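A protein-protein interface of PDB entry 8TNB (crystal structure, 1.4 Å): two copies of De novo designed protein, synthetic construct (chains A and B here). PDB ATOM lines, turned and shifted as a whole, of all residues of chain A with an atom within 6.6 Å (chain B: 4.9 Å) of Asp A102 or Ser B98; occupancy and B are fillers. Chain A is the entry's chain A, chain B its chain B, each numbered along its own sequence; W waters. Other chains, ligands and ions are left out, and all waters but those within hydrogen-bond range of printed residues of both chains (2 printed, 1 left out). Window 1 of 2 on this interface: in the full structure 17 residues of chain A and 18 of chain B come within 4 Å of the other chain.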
ATOM      1  N   ALA A  51      27.187 -14.339 -32.823  1.00  0.00           N
ATOM      2  CA  ALA A  51      26.098 -15.319 -32.863  1.00  0.00           C
ATOM      3  C   ALA A  51      25.611 -15.566 -34.284  1.00  0.00           C
ATOM      4  O   ALA A  51      25.279 -16.707 -34.641  1.00  0.00           O
ATOM      5  CB  ALA A  51      24.939 -14.895 -32.008  1.00  0.00           C
ATOM      6  N   ALA A  97      29.546 -25.103 -29.004  1.00  0.00           N
ATOM      7  CA  ALA A  97      30.014 -23.713 -29.030  1.00  0.00           C
ATOM      8  C   ALA A  97      28.842 -22.765 -29.202  1.00  0.00           C
ATOM      9  O   ALA A  97      28.755 -21.717 -28.550  1.00  0.00           O
ATOM     10  CB  ALA A  97      31.032 -23.492 -30.131  1.00  0.00           C
ATOM     11  N   SER A  98      27.881 -23.161 -30.041  1.00  0.00           N
ATOM     12  CA  SER A  98      26.726 -22.323 -30.294  1.00  0.00           C
ATOM     13  C   SER A  98      25.879 -22.136 -29.036  1.00  0.00           C
ATOM     14  O   SER A  98      25.438 -21.022 -28.729  1.00  0.00           O
ATOM     15  CB  SER A  98      25.929 -22.960 -31.445  1.00  0.00           C
ATOM     16  OG  SER A  98      24.941 -22.063 -31.864  1.00  0.00           O
ATOM     17  N   LYS A  99      25.610 -23.233 -28.316  1.00  0.00           N
ATOM     18  CA  LYS A  99      24.843 -23.170 -27.082  1.00  0.00           C
ATOM     19  C   LYS A  99      25.543 -22.313 -26.041  1.00  0.00           C
ATOM     20  O   LYS A  99      24.902 -21.525 -25.323  1.00  0.00           O
ATOM     21  CB  LYS A  99      24.721 -24.606 -26.558  1.00  0.00           C
ATOM     22  CG  LYS A  99      24.050 -24.753 -25.216  1.00  0.00           C
ATOM     23  CD  LYS A  99      24.060 -26.223 -24.758  1.00  0.00           C
ATOM     24  CE  LYS A  99      25.460 -26.816 -24.719  1.00  0.00           C
ATOM     25  NZ  LYS A  99      25.571 -27.920 -23.725  1.00  0.00           N
ATOM     26  N   THR A 100      26.854 -22.467 -25.951  1.00  0.00           N
ATOM     27  CA  THR A 100      27.623 -21.746 -24.949  1.00  0.00           C
ATOM     28  C   THR A 100      27.686 -20.268 -25.289  1.00  0.00           C
ATOM     29  O   THR A 100      27.532 -19.425 -24.405  1.00  0.00           O
ATOM     30  CB  THR A 100      29.002 -22.382 -24.871  1.00  0.00           C
ATOM     31  OG1 THR A 100      28.863 -23.780 -24.514  1.00  0.00           O
ATOM     32  CG2 THR A 100      29.814 -21.741 -23.828  1.00  0.00           C
ATOM     33  N   LEU A 101      27.882 -19.926 -26.563  1.00  0.00           N
ATOM     34  CA  LEU A 101      27.789 -18.528 -26.958  1.00  0.00           C
ATOM     35  C   LEU A 101      26.413 -17.953 -26.644  1.00  0.00           C
ATOM     36  O   LEU A 101      26.304 -16.802 -26.204  1.00  0.00           O
ATOM     37  CB  LEU A 101      28.107 -18.423 -28.441  1.00  0.00           C
ATOM     38  CG  LEU A 101      28.105 -17.023 -29.015  1.00  0.00           C
ATOM     39  CD1 LEU A 101      29.120 -16.102 -28.288  1.00  0.00           C
ATOM     40  CD2 LEU A 101      28.365 -17.042 -30.486  1.00  0.00           C
ATOM     41  N   ASP A 102      25.332 -18.718 -26.875  1.00  0.00           N
ATOM     42  CA  ASP A 102      23.983 -18.240 -26.548  1.00  0.00           C
ATOM     43  C   ASP A 102      23.897 -17.888 -25.063  1.00  0.00           C
ATOM     44  O   ASP A 102      23.339 -16.854 -24.674  1.00  0.00           O
ATOM     45  CB  ASP A 102      22.935 -19.338 -26.816  1.00  0.00           C
ATOM     46  CG  ASP A 102      22.467 -19.428 -28.271  1.00  0.00           C
ATOM     47  OD1 ASP A 102      22.670 -18.498 -29.071  1.00  0.00           O
ATOM     48  OD2 ASP A 102      21.850 -20.478 -28.600  1.00  0.00           O
ATOM     49  N   THR A 103      24.440 -18.774 -24.211  1.00  0.00           N
ATOM     50  CA  THR A 103      24.438 -18.513 -22.776  1.00  0.00           C
ATOM     51  C   THR A 103      25.167 -17.210 -22.478  1.00  0.00           C
ATOM     52  O   THR A 103      24.682 -16.386 -21.695  1.00  0.00           O
ATOM     53  CB  THR A 103      25.084 -19.675 -22.038  1.00  0.00           C
ATOM     54  OG1 THR A 103      24.269 -20.858 -22.194  1.00  0.00           O
ATOM     55  CG2 THR A 103      25.237 -19.393 -20.539  1.00  0.00           C
ATOM     56  N   ALA A 104      26.286 -16.983 -23.156  1.00  0.00           N
ATOM     57  CA  ALA A 104      27.053 -15.753 -22.944  1.00  0.00           C
ATOM     58  C   ALA A 104      26.278 -14.520 -23.380  1.00  0.00           C
ATOM     59  O   ALA A 104      26.229 -13.518 -22.666  1.00  0.00           O
ATOM     60  CB  ALA A 104      28.401 -15.813 -23.645  1.00  0.00           C
ATOM     61  N   VAL A 105      25.654 -14.575 -24.564  1.00  0.00           N
ATOM     62  CA  VAL A 105      24.840 -13.467 -25.051  1.00  0.00           C
ATOM     63  C   VAL A 105      23.703 -13.129 -24.085  1.00  0.00           C
ATOM     64  O   VAL A 105      23.424 -11.950 -23.806  1.00  0.00           O
ATOM     65  CB  VAL A 105      24.306 -13.841 -26.450  1.00  0.00           C
ATOM     66  CG1 VAL A 105      23.373 -12.783 -26.942  1.00  0.00           C
ATOM     67  CG2 VAL A 105      25.432 -14.009 -27.457  1.00  0.00           C
ATOM     68  N   ALA A 106      23.009 -14.151 -23.572  1.00  0.00           N
ATOM     69  CA  ALA A 106      21.946 -13.901 -22.619  1.00  0.00           C
ATOM     70  C   ALA A 106      22.488 -13.311 -21.334  1.00  0.00           C
ATOM     71  O   ALA A 106      21.864 -12.413 -20.751  1.00  0.00           O
ATOM     72  CB  ALA A 106      21.214 -15.205 -22.299  1.00  0.00           C
ATOM     73  N   ALA A 107      23.613 -13.837 -20.852  1.00  0.00           N
ATOM     74  CA  ALA A 107      24.166 -13.344 -19.596  1.00  0.00           C
ATOM     75  C   ALA A 107      24.560 -11.883 -19.726  1.00  0.00           C
ATOM     76  O   ALA A 107      24.331 -11.078 -18.807  1.00  0.00           O
ATOM     77  CB  ALA A 107      25.355 -14.184 -19.161  1.00  0.00           C
ATOM     78  N   ALA A 119      30.800 -18.684 -19.678  1.00  0.00           N
ATOM     79  CA  ALA A 119      30.321 -19.176 -20.969  1.00  0.00           C
ATOM     80  C   ALA A 119      31.184 -18.656 -22.111  1.00  0.00           C
ATOM     81  O   ALA A 119      31.503 -19.398 -23.046  1.00  0.00           O
ATOM     82  CB  ALA A 119      28.855 -18.793 -21.155  1.00  0.00           C
ATOM     83  N   GLN B  54      14.689 -19.814 -36.060  1.00  0.00           N
ATOM     84  CA  GLN B  54      14.973 -19.880 -34.642  1.00  0.00           C
ATOM     85  C   GLN B  54      16.129 -18.965 -34.274  1.00  0.00           C
ATOM     86  O   GLN B  54      16.065 -18.304 -33.245  1.00  0.00           O
ATOM     87  CB  GLN B  54      15.296 -21.323 -34.246  1.00  0.00           C
ATOM     88  CG  GLN B  54      15.549 -21.514 -32.748  1.00  0.00           C
ATOM     89  CD  GLN B  54      14.321 -21.244 -31.930  1.00  0.00           C
ATOM     90  OE1 GLN B  54      13.334 -21.924 -32.065  1.00  0.00           O
ATOM     91  NE2 GLN B  54      14.357 -20.237 -31.095  1.00  0.00           N
ATOM     92  N   ASP B  58      15.935 -15.947 -31.578  1.00  0.00           N
ATOM     93  CA  ASP B  58      16.904 -15.819 -30.494  1.00  0.00           C
ATOM     94  C   ASP B  58      17.426 -14.387 -30.444  1.00  0.00           C
ATOM     95  O   ASP B  58      17.508 -13.769 -29.379  1.00  0.00           O
ATOM     96  CB  ASP B  58      18.094 -16.751 -30.712  1.00  0.00           C
ATOM     97  CG  ASP B  58      17.768 -18.231 -30.695  1.00  0.00           C
ATOM     98  OD1 ASP B  58      16.685 -18.612 -30.204  1.00  0.00           O
ATOM     99  OD2 ASP B  58      18.660 -19.022 -31.150  1.00  0.00           O
ATOM    100  N   VAL B  94      13.441 -19.453 -25.134  1.00  0.00           N
ATOM    101  CA  VAL B  94      13.809 -19.463 -26.535  1.00  0.00           C
ATOM    102  C   VAL B  94      15.163 -20.120 -26.733  1.00  0.00           C
ATOM    103  O   VAL B  94      15.364 -20.886 -27.679  1.00  0.00           O
ATOM    104  CB  VAL B  94      13.799 -18.005 -27.041  1.00  0.00           C
ATOM    105  CG1 VAL B  94      14.508 -17.863 -28.333  1.00  0.00           C
ATOM    106  CG2 VAL B  94      12.374 -17.498 -27.116  1.00  0.00           C
ATOM    107  N   GLN B  95      16.127 -19.834 -25.864  1.00  0.00           N
ATOM    108  CA  GLN B  95      17.454 -20.435 -26.039  1.00  0.00           C
ATOM    109  C   GLN B  95      17.421 -21.929 -25.744  1.00  0.00           C
ATOM    110  O   GLN B  95      18.173 -22.694 -26.345  1.00  0.00           O
ATOM    111  CB  GLN B  95      18.501 -19.693 -25.215  1.00  0.00           C
ATOM    112  CG  GLN B  95      18.739 -18.291 -25.723  1.00  0.00           C
ATOM    113  CD  GLN B  95      19.963 -17.685 -25.081  1.00  0.00           C
ATOM    114  OE1 GLN B  95      20.350 -18.078 -23.987  1.00  0.00           O
ATOM    115  NE2 GLN B  95      20.609 -16.769 -25.796  1.00  0.00           N
ATOM    116  N   GLU B  96      16.555 -22.348 -24.824  1.00  0.00           N
ATOM    117  CA  GLU B  96      16.365 -23.777 -24.603  1.00  0.00           C
ATOM    118  C   GLU B  96      15.754 -24.450 -25.833  1.00  0.00           C
ATOM    119  O   GLU B  96      16.213 -25.523 -26.263  1.00  0.00           O
ATOM    120  CB  GLU B  96      15.436 -23.983 -23.412  1.00  0.00           C
ATOM    121  CG  GLU B  96      16.058 -23.827 -22.046  1.00  0.00           C
ATOM    122  CD  GLU B  96      14.986 -23.929 -20.958  1.00  0.00           C
ATOM    123  OE1 GLU B  96      13.809 -24.188 -21.300  1.00  0.00           O
ATOM    124  OE2 GLU B  96      15.306 -23.734 -19.766  1.00  0.00           O
ATOM    125  N   ALA B  97      14.750 -23.818 -26.442  1.00  0.00           N
ATOM    126  CA  ALA B  97      14.232 -24.313 -27.725  1.00  0.00           C
ATOM    127  C   ALA B  97      15.318 -24.370 -28.796  1.00  0.00           C
ATOM    128  O   ALA B  97      15.413 -25.326 -29.571  1.00  0.00           O
ATOM    129  CB  ALA B  97      13.090 -23.417 -28.171  1.00  0.00           C
ATOM    130  N   SER B  98      16.155 -23.351 -28.857  1.00  0.00           N
ATOM    131  CA  SER B  98      17.190 -23.304 -29.869  1.00  0.00           C
ATOM    132  C   SER B  98      18.176 -24.450 -29.727  1.00  0.00           C
ATOM    133  O   SER B  98      18.533 -25.088 -30.722  1.00  0.00           O
ATOM    134  CB  SER B  98      17.880 -21.940 -29.752  1.00  0.00           C
ATOM    135  OG  SER B  98      18.794 -21.769 -30.796  1.00  0.00           O
ATOM    136  N   LYS B  99      18.615 -24.739 -28.494  1.00  0.00           N
ATOM    137  CA  LYS B  99      19.555 -25.831 -28.275  1.00  0.00           C
ATOM    138  C   LYS B  99      18.918 -27.171 -28.599  1.00  0.00           C
ATOM    139  O   LYS B  99      19.584 -28.077 -29.113  1.00  0.00           O
ATOM    140  CB  LYS B  99      20.039 -25.811 -26.814  1.00  0.00           C
ATOM    141  CG  LYS B  99      20.287 -27.194 -26.185  1.00  0.00           C
ATOM    142  CD  LYS B  99      20.756 -27.132 -24.715  1.00  0.00           C
ATOM    143  CE  LYS B  99      19.644 -26.767 -23.726  1.00  0.00           C
ATOM    144  NZ  LYS B  99      20.193 -26.173 -22.460  1.00  0.00           N
ATOM    145  N   THR B 100      17.624 -27.295 -28.308  1.00  0.00           N
ATOM    146  CA  THR B 100      16.900 -28.527 -28.584  1.00  0.00           C
ATOM    147  C   THR B 100      16.696 -28.732 -30.073  1.00  0.00           C
ATOM    148  O   THR B 100      16.859 -29.839 -30.594  1.00  0.00           O
ATOM    149  CB  THR B 100      15.584 -28.480 -27.840  1.00  0.00           C
ATOM    150  OG1 THR B 100      15.851 -28.251 -26.446  1.00  0.00           O
ATOM    151  CG2 THR B 100      14.844 -29.795 -27.967  1.00  0.00           C
ATOM    152  N   LEU B 101      16.397 -27.667 -30.796  1.00  0.00           N
ATOM    153  CA  LEU B 101      16.339 -27.791 -32.244  1.00  0.00           C
ATOM    154  C   LEU B 101      17.694 -28.181 -32.811  1.00  0.00           C
ATOM    155  O   LEU B 101      17.783 -28.996 -33.725  1.00  0.00           O
ATOM    156  CB  LEU B 101      15.879 -26.457 -32.826  1.00  0.00           C
ATOM    157  CG  LEU B 101      15.681 -26.436 -34.329  1.00  0.00           C
ATOM    158  CD1 LEU B 101      14.676 -27.484 -34.815  1.00  0.00           C
ATOM    159  CD2 LEU B 101      15.301 -25.041 -34.856  1.00  0.00           C
ATOM    160  N   ASP B 102      18.787 -27.616 -32.277  1.00  0.00           N
ATOM    161  CA  ASP B 102      20.111 -28.028 -32.719  1.00  0.00           C
ATOM    162  C   ASP B 102      20.293 -29.541 -32.590  1.00  0.00           C
ATOM    163  O   ASP B 102      20.820 -30.201 -33.495  1.00  0.00           O
ATOM    164  CB  ASP B 102      21.212 -27.345 -31.896  1.00  0.00           C
ATOM    165  CG  ASP B 102      21.515 -25.924 -32.326  1.00  0.00           C
ATOM    166  OD1 ASP B 102      21.046 -25.488 -33.398  1.00  0.00           O
ATOM    167  OD2 ASP B 102      22.243 -25.248 -31.539  1.00  0.00           O
HETATM  168  O   HOH W   1      20.978 -22.342 -26.560  1.00  0.00           O
HETATM  169  O   HOH W   2      19.804 -19.260 -29.008  1.00  0.00           O
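O of Asp A102 lies within hydrogen-bond range of NE2 of Gln B95 (3.0 Å).
Among the printed residues, merely in contact across the chains: Lys A99 with Lys B99 (3.4 Å), Ala A106 with Gln B95 (3.4 Å) and Asp A102 with Ser B98 (3.98 Å).
Of the 13 printed residues of chain A, 3 touch a printed residue of chain B. Among the printed residues, 4 pairs touch across the chains. Among the printed residues, no Asp or Glu carboxylate lies within 4 Å of a Lys or Arg side-chain nitrogen of the other chain.
The side-chain hydroxyl (OG1) of Thr A103 is in hydrogen-bond range of the backbone carbonyl oxygen (O) of Lys A99 (3.3 Å). The side-chain carboxylate (OD2) of Asp B58 sits at hydrogen-bond distance from the side-chain hydroxyl (OG) of Ser B98.
Water W2 lies within hydrogen-bond range of OD2 of Asp A102, OD2 of Asp B58 and OG of Ser B98. Water W1 lies within hydrogen-bond range of the backbone carbonyl oxygen of Gln B95 (2.8 Å) and the side-chain carboxylate of Asp A102 (2.9 Å).
Printed residues of chain B within 4 Å of Asp A102: Gln B95 (3.0 Å) and Ser B98 (3.98 Å). Of the printed residues of chain B, Ala A106 touches Gln B95 (3.4 Å). Printed residues of chain A within 4 Å of Gln B95: Asp A102 and Ala A106. Of chain A, only Asp A102 (3.98 Å) comes within 4 Å of Ser B98. Of the printed residues of chain A, Lys B99 touches Lys A99 (3.4 Å). The nearest residue of chain B that does not touch Asp A102 is Asp B58 (4.3 Å). The nearest printed residue of chain A that does not touch Gln B95 is Thr A103 (4.2 Å).
Lys B99 touches its own counterpart, Lys A99. Asp A102 touches Ser B98, but with the chains exchanged Ser A98 does not touch Asp B102 (4.2 Å). Positions printed for both chains: 97, 98, 99, 100, 101 and 102.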
